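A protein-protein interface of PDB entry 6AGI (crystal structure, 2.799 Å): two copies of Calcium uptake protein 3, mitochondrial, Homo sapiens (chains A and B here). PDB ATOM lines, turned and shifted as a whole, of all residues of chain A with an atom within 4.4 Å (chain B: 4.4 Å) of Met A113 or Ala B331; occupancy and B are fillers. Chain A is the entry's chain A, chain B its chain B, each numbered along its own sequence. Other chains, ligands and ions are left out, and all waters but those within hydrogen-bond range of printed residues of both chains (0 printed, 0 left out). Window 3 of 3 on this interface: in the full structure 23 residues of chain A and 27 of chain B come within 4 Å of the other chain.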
ATOM      1  N   ILE A 109     -37.016  25.550  10.113  1.00  0.00           N
ATOM      2  CA  ILE A 109     -35.855  26.304  10.550  1.00  0.00           C
ATOM      3  C   ILE A 109     -34.925  25.416  11.370  1.00  0.00           C
ATOM      4  O   ILE A 109     -33.697  25.505  11.247  1.00  0.00           O
ATOM      5  CB  ILE A 109     -36.312  27.567  11.308  1.00  0.00           C
ATOM      6  CG1 ILE A 109     -36.767  28.606  10.278  1.00  0.00           C
ATOM      7  CG2 ILE A 109     -35.186  28.158  12.132  1.00  0.00           C
ATOM      8  CD1 ILE A 109     -37.840  29.580  10.762  1.00  0.00           C
ATOM      9  N   ALA A 110     -35.480  24.508  12.179  1.00  0.00           N
ATOM     10  CA  ALA A 110     -34.636  23.614  12.965  1.00  0.00           C
ATOM     11  C   ALA A 110     -33.874  22.656  12.054  1.00  0.00           C
ATOM     12  O   ALA A 110     -32.642  22.510  12.157  1.00  0.00           O
ATOM     13  CB  ALA A 110     -35.499  22.862  13.970  1.00  0.00           C
ATOM     14  N   PHE A 111     -34.608  22.026  11.129  1.00  0.00           N
ATOM     15  CA  PHE A 111     -34.026  21.158  10.113  1.00  0.00           C
ATOM     16  C   PHE A 111     -32.885  21.856   9.371  1.00  0.00           C
ATOM     17  O   PHE A 111     -31.775  21.316   9.250  1.00  0.00           O
ATOM     18  CB  PHE A 111     -35.141  20.736   9.149  1.00  0.00           C
ATOM     19  CG  PHE A 111     -34.722  19.721   8.123  1.00  0.00           C
ATOM     20  CD1 PHE A 111     -34.732  18.367   8.419  1.00  0.00           C
ATOM     21  CD2 PHE A 111     -34.300  20.124   6.854  1.00  0.00           C
ATOM     22  CE1 PHE A 111     -34.346  17.430   7.473  1.00  0.00           C
ATOM     23  CE2 PHE A 111     -33.899  19.188   5.903  1.00  0.00           C
ATOM     24  CZ  PHE A 111     -33.926  17.842   6.217  1.00  0.00           C
ATOM     25  N   ASN A 112     -33.132  23.079   8.889  1.00  0.00           N
ATOM     26  CA  ASN A 112     -32.095  23.810   8.178  1.00  0.00           C
ATOM     27  C   ASN A 112     -30.940  24.180   9.097  1.00  0.00           C
ATOM     28  O   ASN A 112     -29.794  24.287   8.639  1.00  0.00           O
ATOM     29  CB  ASN A 112     -32.684  25.045   7.519  1.00  0.00           C
ATOM     30  CG  ASN A 112     -33.515  24.700   6.297  1.00  0.00           C
ATOM     31  OD1 ASN A 112     -33.378  23.604   5.727  1.00  0.00           O
ATOM     32  ND2 ASN A 112     -34.385  25.631   5.883  1.00  0.00           N
ATOM     33  N   MET A 113     -31.215  24.397  10.385  1.00  0.00           N
ATOM     34  CA  MET A 113     -30.123  24.606  11.325  1.00  0.00           C
ATOM     35  C   MET A 113     -29.241  23.370  11.430  1.00  0.00           C
ATOM     36  O   MET A 113     -28.057  23.497  11.759  1.00  0.00           O
ATOM     37  CB  MET A 113     -30.665  24.990  12.708  1.00  0.00           C
ATOM     38  CG  MET A 113     -31.060  26.474  12.871  1.00  0.00           C
ATOM     39  SD  MET A 113     -29.704  27.647  12.656  1.00  0.00           S
ATOM     40  CE  MET A 113     -29.087  27.714  14.322  1.00  0.00           C
ATOM     41  N   PHE A 114     -29.776  22.181  11.129  1.00  0.00           N
ATOM     42  CA  PHE A 114     -28.949  20.972  11.141  1.00  0.00           C
ATOM     43  C   PHE A 114     -28.205  20.740   9.822  1.00  0.00           C
ATOM     44  O   PHE A 114     -27.050  20.312   9.834  1.00  0.00           O
ATOM     45  CB  PHE A 114     -29.802  19.735  11.434  1.00  0.00           C
ATOM     46  CG  PHE A 114     -30.028  19.464  12.897  1.00  0.00           C
ATOM     47  CD1 PHE A 114     -29.028  18.917  13.680  1.00  0.00           C
ATOM     48  CD2 PHE A 114     -31.278  19.687  13.471  1.00  0.00           C
ATOM     49  CE1 PHE A 114     -29.252  18.648  15.027  1.00  0.00           C
ATOM     50  CE2 PHE A 114     -31.513  19.411  14.809  1.00  0.00           C
ATOM     51  CZ  PHE A 114     -30.500  18.894  15.589  1.00  0.00           C
ATOM     52  N   ASP A 115     -28.847  21.018   8.682  1.00  0.00           N
ATOM     53  CA  ASP A 115     -28.348  20.664   7.346  1.00  0.00           C
ATOM     54  C   ASP A 115     -27.280  21.662   6.898  1.00  0.00           C
ATOM     55  O   ASP A 115     -27.474  22.479   5.998  1.00  0.00           O
ATOM     56  CB  ASP A 115     -29.517  20.618   6.363  1.00  0.00           C
ATOM     57  CG  ASP A 115     -29.133  20.085   4.985  1.00  0.00           C
ATOM     58  OD1 ASP A 115     -28.093  19.407   4.859  1.00  0.00           O
ATOM     59  OD2 ASP A 115     -29.894  20.342   4.023  1.00  0.00           O
ATOM     60  N   LEU A 130     -23.855  19.183  15.787  1.00  0.00           N
ATOM     61  CA  LEU A 130     -24.536  20.202  16.583  1.00  0.00           C
ATOM     62  C   LEU A 130     -24.798  19.763  18.019  1.00  0.00           C
ATOM     63  O   LEU A 130     -24.846  20.621  18.908  1.00  0.00           O
ATOM     64  CB  LEU A 130     -25.851  20.696  15.954  1.00  0.00           C
ATOM     65  CG  LEU A 130     -25.889  21.441  14.619  1.00  0.00           C
ATOM     66  CD1 LEU A 130     -25.254  20.691  13.432  1.00  0.00           C
ATOM     67  CD2 LEU A 130     -27.350  21.787  14.361  1.00  0.00           C
ATOM     68  N   PHE B 309     -35.662  34.420  15.173  1.00  0.00           N
ATOM     69  CA  PHE B 309     -34.297  34.200  15.663  1.00  0.00           C
ATOM     70  C   PHE B 309     -34.288  33.452  16.999  1.00  0.00           C
ATOM     71  O   PHE B 309     -33.465  32.541  17.212  1.00  0.00           O
ATOM     72  CB  PHE B 309     -33.563  35.529  15.802  1.00  0.00           C
ATOM     73  CG  PHE B 309     -32.067  35.394  15.995  1.00  0.00           C
ATOM     74  CD1 PHE B 309     -31.255  34.888  14.986  1.00  0.00           C
ATOM     75  CD2 PHE B 309     -31.473  35.802  17.186  1.00  0.00           C
ATOM     76  CE1 PHE B 309     -29.880  34.779  15.167  1.00  0.00           C
ATOM     77  CE2 PHE B 309     -30.092  35.707  17.368  1.00  0.00           C
ATOM     78  CZ  PHE B 309     -29.294  35.192  16.354  1.00  0.00           C
ATOM     79  N   ALA B 312     -34.748  29.858  16.451  1.00  0.00           N
ATOM     80  CA  ALA B 312     -33.541  29.240  15.922  1.00  0.00           C
ATOM     81  C   ALA B 312     -32.518  28.957  17.018  1.00  0.00           C
ATOM     82  O   ALA B 312     -31.860  27.912  16.996  1.00  0.00           O
ATOM     83  CB  ALA B 312     -32.937  30.122  14.830  1.00  0.00           C
ATOM     84  N   LEU B 313     -32.331  29.881  17.961  1.00  0.00           N
ATOM     85  CA  LEU B 313     -31.297  29.690  18.981  1.00  0.00           C
ATOM     86  C   LEU B 313     -31.833  29.011  20.248  1.00  0.00           C
ATOM     87  O   LEU B 313     -31.131  28.946  21.276  1.00  0.00           O
ATOM     88  CB  LEU B 313     -30.657  31.039  19.310  1.00  0.00           C
ATOM     89  CG  LEU B 313     -29.680  31.565  18.250  1.00  0.00           C
ATOM     90  CD1 LEU B 313     -28.979  32.808  18.754  1.00  0.00           C
ATOM     91  CD2 LEU B 313     -28.654  30.488  17.842  1.00  0.00           C
ATOM     92  N   GLU B 327     -21.665  31.064  13.907  1.00  0.00           N
ATOM     93  CA  GLU B 327     -23.010  30.520  13.923  1.00  0.00           C
ATOM     94  C   GLU B 327     -24.031  31.542  14.404  1.00  0.00           C
ATOM     95  O   GLU B 327     -25.235  31.309  14.248  1.00  0.00           O
ATOM     96  CB  GLU B 327     -23.053  29.229  14.760  1.00  0.00           C
ATOM     97  CG  GLU B 327     -24.351  28.396  14.544  1.00  0.00           C
ATOM     98  CD  GLU B 327     -24.211  27.235  13.530  1.00  0.00           C
ATOM     99  OE1 GLU B 327     -23.070  26.872  13.147  1.00  0.00           O
ATOM    100  OE2 GLU B 327     -25.260  26.704  13.094  1.00  0.00           O
ATOM    101  N   PHE B 328     -23.599  32.692  14.936  1.00  0.00           N
ATOM    102  CA  PHE B 328     -24.548  33.796  15.074  1.00  0.00           C
ATOM    103  C   PHE B 328     -24.979  34.279  13.698  1.00  0.00           C
ATOM    104  O   PHE B 328     -26.179  34.418  13.420  1.00  0.00           O
ATOM    105  CB  PHE B 328     -23.951  34.945  15.887  1.00  0.00           C
ATOM    106  CG  PHE B 328     -24.857  36.153  15.995  1.00  0.00           C
ATOM    107  CD1 PHE B 328     -24.914  37.101  14.981  1.00  0.00           C
ATOM    108  CD2 PHE B 328     -25.664  36.334  17.099  1.00  0.00           C
ATOM    109  CE1 PHE B 328     -25.742  38.200  15.080  1.00  0.00           C
ATOM    110  CE2 PHE B 328     -26.489  37.428  17.198  1.00  0.00           C
ATOM    111  CZ  PHE B 328     -26.526  38.360  16.190  1.00  0.00           C
ATOM    112  N   LYS B 329     -24.007  34.519  12.812  1.00  0.00           N
ATOM    113  CA  LYS B 329     -24.337  34.897  11.445  1.00  0.00           C
ATOM    114  C   LYS B 329     -25.194  33.827  10.772  1.00  0.00           C
ATOM    115  O   LYS B 329     -26.202  34.130  10.106  1.00  0.00           O
ATOM    116  CB  LYS B 329     -23.062  35.136  10.634  1.00  0.00           C
ATOM    117  CG  LYS B 329     -23.319  34.993   9.141  1.00  0.00           C
ATOM    118  CD  LYS B 329     -22.313  35.714   8.295  1.00  0.00           C
ATOM    119  CE  LYS B 329     -20.952  35.732   8.937  1.00  0.00           C
ATOM    120  NZ  LYS B 329     -19.965  35.845   7.838  1.00  0.00           N
ATOM    121  N   ARG B 330     -24.826  32.555  10.961  1.00  0.00           N
ATOM    122  CA  ARG B 330     -25.549  31.515  10.249  1.00  0.00           C
ATOM    123  C   ARG B 330     -26.966  31.362  10.789  1.00  0.00           C
ATOM    124  O   ARG B 330     -27.912  31.156  10.013  1.00  0.00           O
ATOM    125  CB  ARG B 330     -24.781  30.201  10.338  1.00  0.00           C
ATOM    126  CG  ARG B 330     -25.516  29.100   9.653  1.00  0.00           C
ATOM    127  CD  ARG B 330     -24.683  27.867   9.391  1.00  0.00           C
ATOM    128  NE  ARG B 330     -25.501  26.959   8.597  1.00  0.00           N
ATOM    129  CZ  ARG B 330     -26.433  26.158   9.101  1.00  0.00           C
ATOM    130  NH1 ARG B 330     -26.583  26.060  10.417  1.00  0.00           N
ATOM    131  NH2 ARG B 330     -27.155  25.390   8.291  1.00  0.00           N
ATOM    132  N   ALA B 331     -27.140  31.532  12.106  1.00  0.00           N
ATOM    133  CA  ALA B 331     -28.481  31.534  12.682  1.00  0.00           C
ATOM    134  C   ALA B 331     -29.303  32.681  12.116  1.00  0.00           C
ATOM    135  O   ALA B 331     -30.487  32.509  11.785  1.00  0.00           O
ATOM    136  CB  ALA B 331     -28.407  31.624  14.206  1.00  0.00           C
ATOM    137  N   VAL B 332     -28.679  33.851  11.958  1.00  0.00           N
ATOM    138  CA  VAL B 332     -29.407  34.969  11.378  1.00  0.00           C
ATOM    139  C   VAL B 332     -29.898  34.591   9.992  1.00  0.00           C
ATOM    140  O   VAL B 332     -31.099  34.673   9.704  1.00  0.00           O
ATOM    141  CB  VAL B 332     -28.525  36.234  11.349  1.00  0.00           C
ATOM    142  CG1 VAL B 332     -29.055  37.269  10.343  1.00  0.00           C
ATOM    143  CG2 VAL B 332     -28.437  36.865  12.738  1.00  0.00           C
ATOM    144  N   TYR B 333     -29.009  34.032   9.167  1.00  0.00           N
ATOM    145  CA  TYR B 333     -29.406  33.637   7.816  1.00  0.00           C
ATOM    146  C   TYR B 333     -30.556  32.621   7.825  1.00  0.00           C
ATOM    147  O   TYR B 333     -31.617  32.860   7.230  1.00  0.00           O
ATOM    148  CB  TYR B 333     -28.208  33.085   7.051  1.00  0.00           C
ATOM    149  CG  TYR B 333     -28.614  32.642   5.673  1.00  0.00           C
ATOM    150  CD1 TYR B 333     -29.358  33.481   4.847  1.00  0.00           C
ATOM    151  CD2 TYR B 333     -28.239  31.395   5.186  1.00  0.00           C
ATOM    152  CE1 TYR B 333     -29.746  33.077   3.586  1.00  0.00           C
ATOM    153  CE2 TYR B 333     -28.614  30.983   3.927  1.00  0.00           C
ATOM    154  CZ  TYR B 333     -29.370  31.824   3.126  1.00  0.00           C
ATOM    155  OH  TYR B 333     -29.743  31.418   1.861  1.00  0.00           O
ATOM    156  N   VAL B 334     -30.372  31.482   8.504  1.00  0.00           N
ATOM    157  CA  VAL B 334     -31.348  30.407   8.361  1.00  0.00           C
ATOM    158  C   VAL B 334     -32.686  30.799   8.975  1.00  0.00           C
ATOM    159  O   VAL B 334     -33.751  30.371   8.495  1.00  0.00           O
ATOM    160  CB  VAL B 334     -30.802  29.099   8.976  1.00  0.00           C
ATOM    161  CG1 VAL B 334     -31.939  28.186   9.383  1.00  0.00           C
ATOM    162  CG2 VAL B 334     -29.927  28.371   7.974  1.00  0.00           C
ATOM    163  N   ALA B 335     -32.676  31.635  10.019  1.00  0.00           N
ATOM    164  CA  ALA B 335     -33.926  32.101  10.611  1.00  0.00           C
ATOM    165  C   ALA B 335     -34.586  33.176   9.759  1.00  0.00           C
ATOM    166  O   ALA B 335     -35.794  33.104   9.494  1.00  0.00           O
ATOM    167  CB  ALA B 335     -33.697  32.614  12.019  1.00  0.00           C
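The backbone carbonyl oxygen (O) of Met A113 sits at hydrogen-bond distance from the guanidinium group (NH1) of Arg B330, 3.2 Å away. The backbone carbonyl oxygen of Asn A112 is in hydrogen-bond range of the guanidinium group of Arg B330, 2.9 Å away.
The side-chain carboxylate (OE2) of Glu B327 is in salt-bridge range of the guanidinium group (NH1) of Arg B330 (3.1 Å).
Among the printed residues, merely in contact across the chains: Ile A109 with Val B334 (3.7 Å), Asn A112 with Val B334 (3.7 Å), Met A113 with Ala B312 (3.9 Å), Met A113 with Ala B331 (3.97 Å), Met A113 with Val B334 (3.98 Å) and Asp A115 with Arg B330 (3.7 Å).
Printed residues of chain B within 4 Å of Met A113: Ala B312 (3.9 Å), Arg B330 (3.2 Å), Ala B331 (3.97 Å) and Val B334 (3.98 Å). Printed residues of chain A within 4 Å of Arg B330: Asn A112, Met A113 and Asp A115. Of the printed residues of chain B, Asn A112 touches Arg B330 (2.9 Å) and Val B334 (3.7 Å). The nearest printed residue of chain A that does not touch Ala B331 is Ile A109 (6.4 Å).
Of the 8 printed residues of chain A, 4 touch a printed residue of chain B. Hydrophobic or aromatic side chains of chain A within 4 Å of the printed part of chain B: Ile A109 and Met A113. Printed residues of chain B that touch a printed residue of chain A: Ala B312, Arg B330, Ala B331 and Val B334. Hydrophobic or aromatic side chains of chain B that line the printed part of chain A: Ala B331 and Val B334.
No position is printed for both chains.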
